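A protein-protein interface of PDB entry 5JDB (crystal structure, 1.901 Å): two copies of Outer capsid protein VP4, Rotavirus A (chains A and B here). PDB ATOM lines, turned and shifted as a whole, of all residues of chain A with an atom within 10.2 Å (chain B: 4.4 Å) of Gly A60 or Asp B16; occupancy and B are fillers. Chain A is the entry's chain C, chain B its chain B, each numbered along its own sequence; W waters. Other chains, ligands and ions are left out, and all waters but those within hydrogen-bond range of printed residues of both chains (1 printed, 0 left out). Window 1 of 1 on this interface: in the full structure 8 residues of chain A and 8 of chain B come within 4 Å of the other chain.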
ATOM      1  N   VAL A  28       0.041  20.146 -33.351  1.00  0.00           N
ATOM      2  CA  VAL A  28      -1.371  19.850 -33.582  1.00  0.00           C
ATOM      3  C   VAL A  28      -1.989  20.999 -34.376  1.00  0.00           C
ATOM      4  O   VAL A  28      -1.915  22.156 -33.962  1.00  0.00           O
ATOM      5  CB  VAL A  28      -2.116  19.651 -32.259  1.00  0.00           C
ATOM      6  CG1 VAL A  28      -3.608  19.334 -32.497  1.00  0.00           C
ATOM      7  CG2 VAL A  28      -1.433  18.545 -31.445  1.00  0.00           C
ATOM      8  N   GLU A  31      -8.088  20.062 -33.378  1.00  0.00           N
ATOM      9  CA  GLU A  31      -8.734  18.947 -32.675  1.00  0.00           C
ATOM     10  C   GLU A  31     -10.233  19.046 -32.896  1.00  0.00           C
ATOM     11  O   GLU A  31     -10.810  20.105 -32.661  1.00  0.00           O
ATOM     12  CB  GLU A  31      -8.464  18.994 -31.165  1.00  0.00           C
ATOM     13  CG  GLU A  31      -7.061  18.699 -30.705  1.00  0.00           C
ATOM     14  CD  GLU A  31      -6.895  18.957 -29.208  1.00  0.00           C
ATOM     15  OE1 GLU A  31      -5.747  19.176 -28.765  1.00  0.00           O
ATOM     16  OE2 GLU A  31      -7.914  18.977 -28.481  1.00  0.00           O
ATOM     17  N   SER A  32     -10.875  17.959 -33.311  1.00  0.00           N
ATOM     18  CA  SER A  32     -12.309  18.001 -33.582  1.00  0.00           C
ATOM     19  C   SER A  32     -13.018  16.824 -32.927  1.00  0.00           C
ATOM     20  O   SER A  32     -12.590  15.687 -33.106  1.00  0.00           O
ATOM     21  CB  SER A  32     -12.554  17.998 -35.098  1.00  0.00           C
ATOM     22  OG  SER A  32     -13.935  18.137 -35.398  1.00  0.00           O
ATOM     23  N   THR A  33     -14.083  17.085 -32.162  1.00  0.00           N
ATOM     24  CA  THR A  33     -14.918  16.006 -31.613  1.00  0.00           C
ATOM     25  C   THR A  33     -16.378  16.415 -31.357  1.00  0.00           C
ATOM     26  O   THR A  33     -16.704  17.595 -31.277  1.00  0.00           O
ATOM     27  CB  THR A  33     -14.340  15.444 -30.283  1.00  0.00           C
ATOM     28  OG1 THR A  33     -15.084  14.280 -29.881  1.00  0.00           O
ATOM     29  CG2 THR A  33     -14.381  16.483 -29.172  1.00  0.00           C
ATOM     30  N   ASN A  35     -17.717  14.449 -28.876  1.00  0.00           N
ATOM     31  CA  ASN A  35     -17.682  13.735 -27.596  1.00  0.00           C
ATOM     32  C   ASN A  35     -18.622  12.542 -27.509  1.00  0.00           C
ATOM     33  O   ASN A  35     -18.968  12.108 -26.410  1.00  0.00           O
ATOM     34  CB  ASN A  35     -17.975  14.688 -26.435  1.00  0.00           C
ATOM     35  CG  ASN A  35     -16.803  15.600 -26.122  1.00  0.00           C
ATOM     36  OD1 ASN A  35     -15.721  15.136 -25.754  1.00  0.00           O
ATOM     37  ND2 ASN A  35     -17.017  16.894 -26.245  1.00  0.00           N
ATOM     38  N   TRP A  39     -13.636  11.634 -32.798  1.00  0.00           N
ATOM     39  CA  TRP A  39     -12.503  12.441 -32.357  1.00  0.00           C
ATOM     40  C   TRP A  39     -11.463  12.410 -33.462  1.00  0.00           C
ATOM     41  O   TRP A  39     -10.989  11.329 -33.823  1.00  0.00           O
ATOM     42  CB  TRP A  39     -11.860  11.906 -31.079  1.00  0.00           C
ATOM     43  CG  TRP A  39     -12.615  12.080 -29.791  1.00  0.00           C
ATOM     44  CD1 TRP A  39     -12.335  12.967 -28.794  1.00  0.00           C
ATOM     45  CD2 TRP A  39     -13.728  11.303 -29.335  1.00  0.00           C
ATOM     46  NE1 TRP A  39     -13.211  12.810 -27.760  1.00  0.00           N
ATOM     47  CE2 TRP A  39     -14.081  11.794 -28.063  1.00  0.00           C
ATOM     48  CE3 TRP A  39     -14.469  10.253 -29.886  1.00  0.00           C
ATOM     49  CZ2 TRP A  39     -15.147  11.275 -27.331  1.00  0.00           C
ATOM     50  CZ3 TRP A  39     -15.533   9.739 -29.160  1.00  0.00           C
ATOM     51  CH2 TRP A  39     -15.857  10.245 -27.892  1.00  0.00           C
ATOM     52  N   ALA A  41      -7.788  14.427 -34.581  1.00  0.00           N
ATOM     53  CA  ALA A  41      -6.753  15.420 -34.377  1.00  0.00           C
ATOM     54  C   ALA A  41      -5.807  15.323 -35.552  1.00  0.00           C
ATOM     55  O   ALA A  41      -5.448  14.220 -35.961  1.00  0.00           O
ATOM     56  CB  ALA A  41      -6.024  15.185 -33.060  1.00  0.00           C
ATOM     57  N   TYR A  56       2.172  14.494 -28.283  1.00  0.00           N
ATOM     58  CA  TYR A  56       1.271  15.604 -28.611  1.00  0.00           C
ATOM     59  C   TYR A  56       0.201  15.758 -27.540  1.00  0.00           C
ATOM     60  O   TYR A  56      -0.192  14.786 -26.895  1.00  0.00           O
ATOM     61  CB  TYR A  56       0.591  15.409 -29.978  1.00  0.00           C
ATOM     62  CG  TYR A  56       1.540  15.242 -31.140  1.00  0.00           C
ATOM     63  CD1 TYR A  56       1.981  16.343 -31.870  1.00  0.00           C
ATOM     64  CD2 TYR A  56       2.002  13.986 -31.506  1.00  0.00           C
ATOM     65  CE1 TYR A  56       2.857  16.189 -32.930  1.00  0.00           C
ATOM     66  CE2 TYR A  56       2.880  13.822 -32.568  1.00  0.00           C
ATOM     67  CZ  TYR A  56       3.302  14.932 -33.277  1.00  0.00           C
ATOM     68  OH  TYR A  56       4.171  14.783 -34.337  1.00  0.00           O
ATOM     69  N   THR A  57      -0.270  16.984 -27.347  1.00  0.00           N
ATOM     70  CA  THR A  57      -1.404  17.207 -26.464  1.00  0.00           C
ATOM     71  C   THR A  57      -2.652  17.172 -27.320  1.00  0.00           C
ATOM     72  O   THR A  57      -2.811  18.001 -28.211  1.00  0.00           O
ATOM     73  CB  THR A  57      -1.307  18.550 -25.715  1.00  0.00           C
ATOM     74  OG1 THR A  57      -0.202  18.510 -24.805  1.00  0.00           O
ATOM     75  CG2 THR A  57      -2.571  18.811 -24.933  1.00  0.00           C
ATOM     76  N   VAL A  58      -3.519  16.190 -27.093  1.00  0.00           N
ATOM     77  CA  VAL A  58      -4.765  16.131 -27.840  1.00  0.00           C
ATOM     78  C   VAL A  58      -5.931  15.800 -26.915  1.00  0.00           C
ATOM     79  O   VAL A  58      -5.855  14.873 -26.091  1.00  0.00           O
ATOM     80  CB  VAL A  58      -4.719  15.098 -28.991  1.00  0.00           C
ATOM     81  CG1 VAL A  58      -3.880  15.608 -30.141  1.00  0.00           C
ATOM     82  CG2 VAL A  58      -4.207  13.755 -28.492  1.00  0.00           C
ATOM     83  N   PHE A  59      -6.996  16.580 -27.059  1.00  0.00           N
ATOM     84  CA  PHE A  59      -8.187  16.475 -26.225  1.00  0.00           C
ATOM     85  C   PHE A  59      -7.815  16.475 -24.746  1.00  0.00           C
ATOM     86  O   PHE A  59      -8.413  15.760 -23.941  1.00  0.00           O
ATOM     87  CB  PHE A  59      -8.990  15.229 -26.606  1.00  0.00           C
ATOM     88  CG  PHE A  59      -9.366  15.197 -28.066  1.00  0.00           C
ATOM     89  CD1 PHE A  59     -10.344  16.051 -28.563  1.00  0.00           C
ATOM     90  CD2 PHE A  59      -8.706  14.363 -28.952  1.00  0.00           C
ATOM     91  CE1 PHE A  59     -10.672  16.048 -29.910  1.00  0.00           C
ATOM     92  CE2 PHE A  59      -9.032  14.357 -30.300  1.00  0.00           C
ATOM     93  CZ  PHE A  59     -10.016  15.196 -30.777  1.00  0.00           C
ATOM     94  N   GLY A  60      -6.814  17.281 -24.408  1.00  0.00           N
ATOM     95  CA  GLY A  60      -6.407  17.471 -23.029  1.00  0.00           C
ATOM     96  C   GLY A  60      -5.481  16.398 -22.463  1.00  0.00           C
ATOM     97  O   GLY A  60      -5.099  16.466 -21.295  1.00  0.00           O
ATOM     98  N   GLU A  61      -5.123  15.412 -23.280  1.00  0.00           N
ATOM     99  CA  GLU A  61      -4.238  14.335 -22.829  1.00  0.00           C
ATOM    100  C   GLU A  61      -2.908  14.322 -23.582  1.00  0.00           C
ATOM    101  O   GLU A  61      -2.836  14.719 -24.739  1.00  0.00           O
ATOM    102  CB  GLU A  61      -4.919  12.969 -22.997  1.00  0.00           C
ATOM    103  CG  GLU A  61      -6.389  12.940 -22.585  1.00  0.00           C
ATOM    104  CD  GLU A  61      -7.075  11.633 -22.952  1.00  0.00           C
ATOM    105  OE1 GLU A  61      -6.407  10.744 -23.523  1.00  0.00           O
ATOM    106  OE2 GLU A  61      -8.285  11.495 -22.677  1.00  0.00           O
ATOM    107  N   ASN A  62      -1.857  13.851 -22.916  1.00  0.00           N
ATOM    108  CA  ASN A  62      -0.593  13.553 -23.595  1.00  0.00           C
ATOM    109  C   ASN A  62      -0.678  12.226 -24.333  1.00  0.00           C
ATOM    110  O   ASN A  62      -0.875  11.181 -23.714  1.00  0.00           O
ATOM    111  CB  ASN A  62       0.575  13.498 -22.603  1.00  0.00           C
ATOM    112  CG  ASN A  62       0.947  14.857 -22.062  1.00  0.00           C
ATOM    113  OD1 ASN A  62       0.671  15.890 -22.681  1.00  0.00           O
ATOM    114  ND2 ASN A  62       1.579  14.868 -20.892  1.00  0.00           N
ATOM    115  N   LYS A  63      -0.556  12.266 -25.653  1.00  0.00           N
ATOM    116  CA  LYS A  63      -0.573  11.045 -26.448  1.00  0.00           C
ATOM    117  C   LYS A  63       0.742  10.879 -27.188  1.00  0.00           C
ATOM    118  O   LYS A  63       1.332  11.863 -27.647  1.00  0.00           O
ATOM    119  CB  LYS A  63      -1.729  11.060 -27.453  1.00  0.00           C
ATOM    120  CG  LYS A  63      -3.097  10.686 -26.879  1.00  0.00           C
ATOM    121  CD  LYS A  63      -3.156   9.212 -26.469  1.00  0.00           C
ATOM    122  CE  LYS A  63      -4.404   8.903 -25.663  1.00  0.00           C
ATOM    123  NZ  LYS A  63      -4.456   7.459 -25.292  1.00  0.00           N
ATOM    124  N   ARG A  81     -10.367   8.320 -33.630  1.00  0.00           N
ATOM    125  CA  ARG A  81     -10.997   7.277 -32.831  1.00  0.00           C
ATOM    126  C   ARG A  81     -12.491   7.577 -32.740  1.00  0.00           C
ATOM    127  O   ARG A  81     -12.902   8.741 -32.836  1.00  0.00           O
ATOM    128  CB  ARG A  81     -10.378   7.190 -31.439  1.00  0.00           C
ATOM    129  CG  ARG A  81     -10.518   8.465 -30.652  1.00  0.00           C
ATOM    130  CD  ARG A  81      -9.975   8.335 -29.244  1.00  0.00           C
ATOM    131  NE  ARG A  81     -10.318   9.523 -28.476  1.00  0.00           N
ATOM    132  CZ  ARG A  81      -9.876   9.781 -27.252  1.00  0.00           C
ATOM    133  NH1 ARG A  81      -9.077   8.916 -26.639  1.00  0.00           N
ATOM    134  NH2 ARG A  81     -10.244  10.904 -26.637  1.00  0.00           N
ATOM    135  N   SER A  84     -13.732   7.128 -26.783  1.00  0.00           N
ATOM    136  CA  SER A  84     -12.656   7.575 -25.904  1.00  0.00           C
ATOM    137  C   SER A  84     -11.895   6.409 -25.280  1.00  0.00           C
ATOM    138  O   SER A  84     -10.866   6.622 -24.635  1.00  0.00           O
ATOM    139  CB  SER A  84     -13.201   8.493 -24.822  1.00  0.00           C
ATOM    140  OG  SER A  84     -14.449   8.015 -24.338  1.00  0.00           O
ATOM    141  N   PHE A  88      -5.955   5.934 -30.847  1.00  0.00           N
ATOM    142  CA  PHE A  88      -5.958   6.653 -32.108  1.00  0.00           C
ATOM    143  C   PHE A  88      -5.220   5.853 -33.161  1.00  0.00           C
ATOM    144  O   PHE A  88      -4.199   5.243 -32.855  1.00  0.00           O
ATOM    145  CB  PHE A  88      -5.297   8.023 -31.961  1.00  0.00           C
ATOM    146  CG  PHE A  88      -6.157   9.050 -31.291  1.00  0.00           C
ATOM    147  CD1 PHE A  88      -6.024   9.306 -29.936  1.00  0.00           C
ATOM    148  CD2 PHE A  88      -7.076   9.785 -32.025  1.00  0.00           C
ATOM    149  CE1 PHE A  88      -6.815  10.260 -29.321  1.00  0.00           C
ATOM    150  CE2 PHE A  88      -7.867  10.732 -31.420  1.00  0.00           C
ATOM    151  CZ  PHE A  88      -7.737  10.967 -30.057  1.00  0.00           C
ATOM    152  N   ILE A 136     -11.171  22.806 -32.118  1.00  0.00           N
ATOM    153  CA  ILE A 136     -10.146  23.708 -31.613  1.00  0.00           C
ATOM    154  C   ILE A 136      -9.147  23.888 -32.737  1.00  0.00           C
ATOM    155  O   ILE A 136      -8.616  22.909 -33.242  1.00  0.00           O
ATOM    156  CB  ILE A 136      -9.426  23.166 -30.355  1.00  0.00           C
ATOM    157  CG1 ILE A 136     -10.421  22.878 -29.235  1.00  0.00           C
ATOM    158  CG2 ILE A 136      -8.348  24.146 -29.875  1.00  0.00           C
ATOM    159  CD1 ILE A 136      -9.831  21.985 -28.143  1.00  0.00           C
ATOM    160  N   HIS A 138      -5.606  25.743 -34.031  1.00  0.00           N
ATOM    161  CA  HIS A 138      -4.397  26.289 -33.420  1.00  0.00           C
ATOM    162  C   HIS A 138      -3.633  27.235 -34.341  1.00  0.00           C
ATOM    163  O   HIS A 138      -2.516  27.654 -34.025  1.00  0.00           O
ATOM    164  CB  HIS A 138      -3.469  25.146 -32.975  1.00  0.00           C
ATOM    165  CG  HIS A 138      -4.031  24.313 -31.862  1.00  0.00           C
ATOM    166  ND1 HIS A 138      -4.947  23.304 -32.076  1.00  0.00           N
ATOM    167  CD2 HIS A 138      -3.803  24.335 -30.527  1.00  0.00           C
ATOM    168  CE1 HIS A 138      -5.261  22.741 -30.920  1.00  0.00           C
ATOM    169  NE2 HIS A 138      -4.581  23.348 -29.966  1.00  0.00           N
ATOM    170  N   PRO B  14     -14.075  23.201 -24.381  1.00  0.00           N
ATOM    171  CA  PRO B  14     -13.914  21.777 -24.688  1.00  0.00           C
ATOM    172  C   PRO B  14     -13.763  20.939 -23.426  1.00  0.00           C
ATOM    173  O   PRO B  14     -13.302  21.441 -22.397  1.00  0.00           O
ATOM    174  CB  PRO B  14     -12.635  21.739 -25.525  1.00  0.00           C
ATOM    175  CG  PRO B  14     -11.873  22.980 -25.107  1.00  0.00           C
ATOM    176  CD  PRO B  14     -12.928  24.013 -24.830  1.00  0.00           C
ATOM    177  N   ILE B  15     -14.156  19.673 -23.516  1.00  0.00           N
ATOM    178  CA  ILE B  15     -13.928  18.715 -22.441  1.00  0.00           C
ATOM    179  C   ILE B  15     -12.430  18.467 -22.267  1.00  0.00           C
ATOM    180  O   ILE B  15     -11.713  18.331 -23.266  1.00  0.00           O
ATOM    181  CB  ILE B  15     -14.629  17.362 -22.723  1.00  0.00           C
ATOM    182  CG1 ILE B  15     -16.143  17.540 -22.835  1.00  0.00           C
ATOM    183  CG2 ILE B  15     -14.275  16.340 -21.654  1.00  0.00           C
ATOM    184  CD1 ILE B  15     -16.802  17.894 -21.526  1.00  0.00           C
ATOM    185  N   ASP B  16     -11.990  18.459 -21.002  1.00  0.00           N
ATOM    186  CA  ASP B  16     -10.663  18.013 -20.558  1.00  0.00           C
ATOM    187  C   ASP B  16      -9.613  19.127 -20.653  1.00  0.00           C
ATOM    188  O   ASP B  16      -8.432  18.853 -20.792  1.00  0.00           O
ATOM    189  CB  ASP B  16     -10.213  16.778 -21.354  1.00  0.00           C
ATOM    190  CG  ASP B  16      -9.218  15.915 -20.592  1.00  0.00           C
ATOM    191  OD1 ASP B  16      -8.358  15.279 -21.236  1.00  0.00           O
ATOM    192  OD2 ASP B  16      -9.304  15.863 -19.350  1.00  0.00           O
ATOM    193  N   TYR B  17     -10.061  20.382 -20.561  1.00  0.00           N
ATOM    194  CA  TYR B  17      -9.152  21.527 -20.494  1.00  0.00           C
ATOM    195  C   TYR B  17      -9.507  22.448 -19.334  1.00  0.00           C
ATOM    196  O   TYR B  17     -10.677  22.759 -19.121  1.00  0.00           O
ATOM    197  CB  TYR B  17      -9.196  22.325 -21.793  1.00  0.00           C
ATOM    198  CG  TYR B  17      -8.571  21.640 -22.981  1.00  0.00           C
ATOM    199  CD1 TYR B  17      -9.324  20.826 -23.813  1.00  0.00           C
ATOM    200  CD2 TYR B  17      -7.227  21.836 -23.290  1.00  0.00           C
ATOM    201  CE1 TYR B  17      -8.754  20.211 -24.910  1.00  0.00           C
ATOM    202  CE2 TYR B  17      -6.651  21.228 -24.381  1.00  0.00           C
ATOM    203  CZ  TYR B  17      -7.416  20.418 -25.189  1.00  0.00           C
ATOM    204  OH  TYR B  17      -6.843  19.806 -26.284  1.00  0.00           O
ATOM    205  N   LEU B 104     -12.982  23.476 -15.042  1.00  0.00           N
ATOM    206  CA  LEU B 104     -12.696  22.315 -15.875  1.00  0.00           C
ATOM    207  C   LEU B 104     -13.951  21.475 -16.086  1.00  0.00           C
ATOM    208  O   LEU B 104     -14.724  21.278 -15.155  1.00  0.00           O
ATOM    209  CB  LEU B 104     -11.596  21.453 -15.236  1.00  0.00           C
ATOM    210  CG  LEU B 104     -11.488  20.009 -15.740  1.00  0.00           C
ATOM    211  CD1 LEU B 104     -10.906  19.977 -17.159  1.00  0.00           C
ATOM    212  CD2 LEU B 104     -10.666  19.131 -14.776  1.00  0.00           C
ATOM    213  N   LYS B 105     -14.140  20.995 -17.312  1.00  0.00           N
ATOM    214  CA  LYS B 105     -15.181  20.034 -17.645  1.00  0.00           C
ATOM    215  C   LYS B 105     -14.529  18.666 -17.819  1.00  0.00           C
ATOM    216  O   LYS B 105     -13.757  18.453 -18.755  1.00  0.00           O
ATOM    217  CB  LYS B 105     -15.936  20.446 -18.915  1.00  0.00           C
ATOM    218  CG  LYS B 105     -16.907  21.602 -18.684  1.00  0.00           C
ATOM    219  CD  LYS B 105     -17.242  22.392 -19.955  1.00  0.00           C
ATOM    220  CE  LYS B 105     -17.901  21.528 -21.014  1.00  0.00           C
ATOM    221  NZ  LYS B 105     -18.748  22.343 -21.936  1.00  0.00           N
ATOM    222  N   TYR B 106     -14.829  17.742 -16.912  1.00  0.00           N
ATOM    223  CA  TYR B 106     -14.213  16.429 -16.977  1.00  0.00           C
ATOM    224  C   TYR B 106     -15.028  15.361 -16.261  1.00  0.00           C
ATOM    225  O   TYR B 106     -15.513  15.593 -15.157  1.00  0.00           O
ATOM    226  CB  TYR B 106     -12.816  16.468 -16.374  1.00  0.00           C
ATOM    227  CG  TYR B 106     -12.185  15.100 -16.273  1.00  0.00           C
ATOM    228  CD1 TYR B 106     -11.642  14.479 -17.393  1.00  0.00           C
ATOM    229  CD2 TYR B 106     -12.149  14.417 -15.060  1.00  0.00           C
ATOM    230  CE1 TYR B 106     -11.072  13.221 -17.307  1.00  0.00           C
ATOM    231  CE2 TYR B 106     -11.583  13.157 -14.965  1.00  0.00           C
ATOM    232  CZ  TYR B 106     -11.047  12.567 -16.091  1.00  0.00           C
ATOM    233  OH  TYR B 106     -10.478  11.318 -15.994  1.00  0.00           O
ATOM    234  N   PRO B 145      -4.368  22.056 -20.772  1.00  0.00           N
ATOM    235  CA  PRO B 145      -4.885  20.682 -20.796  1.00  0.00           C
ATOM    236  C   PRO B 145      -4.883  20.033 -19.403  1.00  0.00           C
ATOM    237  O   PRO B 145      -4.040  20.369 -18.586  1.00  0.00           O
ATOM    238  CB  PRO B 145      -3.925  19.963 -21.749  1.00  0.00           C
ATOM    239  CG  PRO B 145      -2.652  20.770 -21.680  1.00  0.00           C
ATOM    240  CD  PRO B 145      -3.061  22.185 -21.446  1.00  0.00           C
ATOM    241  N   ARG B 146      -5.807  19.117 -19.136  1.00  0.00           N
ATOM    242  CA  ARG B 146      -5.869  18.483 -17.824  1.00  0.00           C
ATOM    243  C   ARG B 146      -4.584  17.708 -17.558  1.00  0.00           C
ATOM    244  O   ARG B 146      -4.163  17.594 -16.415  1.00  0.00           O
ATOM    245  CB  ARG B 146      -7.085  17.561 -17.732  1.00  0.00           C
ATOM    246  CG  ARG B 146      -7.474  17.158 -16.325  1.00  0.00           C
ATOM    247  CD  ARG B 146      -8.685  16.230 -16.359  1.00  0.00           C
ATOM    248  NE  ARG B 146      -8.269  14.929 -16.807  1.00  0.00           N
ATOM    249  CZ  ARG B 146      -7.919  13.911 -16.018  1.00  0.00           C
ATOM    250  NH1 ARG B 146      -7.890  13.988 -14.667  1.00  0.00           N
ATOM    251  NH2 ARG B 146      -7.571  12.790 -16.632  1.00  0.00           N
ATOM    252  N   SER B 147      -3.964  17.175 -18.607  1.00  0.00           N
ATOM    253  CA  SER B 147      -2.633  16.565 -18.475  1.00  0.00           C
ATOM    254  C   SER B 147      -1.624  17.421 -17.682  1.00  0.00           C
ATOM    255  O   SER B 147      -0.737  16.877 -17.018  1.00  0.00           O
ATOM    256  CB  SER B 147      -2.052  16.264 -19.858  1.00  0.00           C
ATOM    257  OG  SER B 147      -1.817  17.463 -20.578  1.00  0.00           O
HETATM  258  O   HOH W   1     -14.815  18.654 -26.163  1.00  0.00           O
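The side-chain carboxylate (OD1) of Asp B16 sits close to the backbone carbonyl oxygen (O) of Phe A59 (2.7 Å). OE2 of Glu A31 sits at hydrogen-bond distance from OH of Tyr B17 (2.6 Å). The side-chain hydroxyl (OH) of Tyr B17 sits at hydrogen-bond distance from the backbone NH (N) of Phe A59 (3.3 Å). The side-chain hydroxyl (OH) of Tyr B17 lies within hydrogen-bond range of the backbone NH (N) of Gly A60 (3.1 Å). The backbone carbonyl oxygen (O) of Gly A60 sits at hydrogen-bond distance from the backbone NH (N) of Arg B146 (3.5 Å). The backbone NH of Ser B147 is in hydrogen-bond range of the backbone carbonyl oxygen of Gly A60, 3.0 Å away. The side-chain carboxylate (OD1) of Asp B16 sits close to the backbone carbonyl oxygen (O) of Gly A60 (3.5 Å).
N of Asp B16 is in hydrogen-bond range of O of Lys B105 (2.9 Å). The side-chain carboxylate of Asp B16 is in salt-bridge range of the guanidinium group of Arg B146, at 2.9 Å. The side-chain hydroxyl of Tyr B106 lies within hydrogen-bond range of the guanidinium group of Arg B146 (3.3 Å). The backbone NH of Ile A136 is in hydrogen-bond range of the backbone carbonyl oxygen of Glu A31 (2.8 Å). OG1 of Thr A33 is in hydrogen-bond range of N of Asn A35 (2.8 Å). The side-chain hydroxyl of Thr A57 sits at hydrogen-bond distance from the side-chain amide oxygen of Asn A62 (3.5 Å).
Among the printed residues, pairs that only touch across the chains: Asn A35 with Ile B15 (3.6 Å), Thr A57 with Pro B145 (3.6 Å), Gly A60 with Pro B145 (3.7 Å), Glu A61 with Asp B16 (3.3 Å), Asn A62 with Ser B147 (3.6 Å), Ile A136 with Pro B14 (3.8 Å) and Ile A136 with Tyr B17 (3.8 Å).
Printed residues of chain B within 4 Å of Glu A31: Tyr B17 (2.6 Å). Of the printed residues of chain B, Asn A35 touches Ile B15 (3.6 Å). Printed residues of chain B within 4 Å of Phe A59: Asp B16 (2.7 Å) and Tyr B17 (3.3 Å). Of the printed residues of chain B, Gly A60 touches Asp B16 (3.3 Å), Tyr B17 (3.1 Å), Pro B145 (3.7 Å), Arg B146 (3.5 Å) and Ser B147 (3.0 Å). Printed residues of chain B within 4 Å of Glu A61: Asp B16. Of the printed residues of chain A, Pro B14 touches Ile A136 (3.8 Å). Ile B15 touches one residue of chain A. Asp B16 touches just these residues of chain A: Phe A59 (2.7 Å), Gly A60 (3.3 Å) and Glu A61 (3.3 Å). Tyr B17 touches four residues of chain A. Pro B145 touches just these residues of chain A: Thr A57 (3.6 Å) and Gly A60 (3.7 Å). Ser B147 touches two residues of chain A. The nearest printed residue of chain B that does not touch Gly A60 is Ile B15 (5.1 Å). The nearest residue of chain A that does not touch Asp B16 is Val A58 (5.5 Å).
Printed residues of chain A that touch a printed residue of chain B: Glu A31, Asn A35, Thr A57, Phe A59, Gly A60, Glu A61, Asn A62 and Ile A136. Hydrophobic or aromatic side chains of chain B that line the printed part of chain A: Pro B14, Ile B15, Tyr B17 and Pro B145. Among the printed residues, 14 pairs touch across the chains.
No position is printed for both chains. Of the 14 pairs that touch across the chains among the printed residues, none has its exchanged pair printed and touching as well.
Water W1 lies within hydrogen-bond range of the side-chain amide nitrogen of Asn A35 (2.8 Å) and the backbone NH of Ile B15 (2.9 Å).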
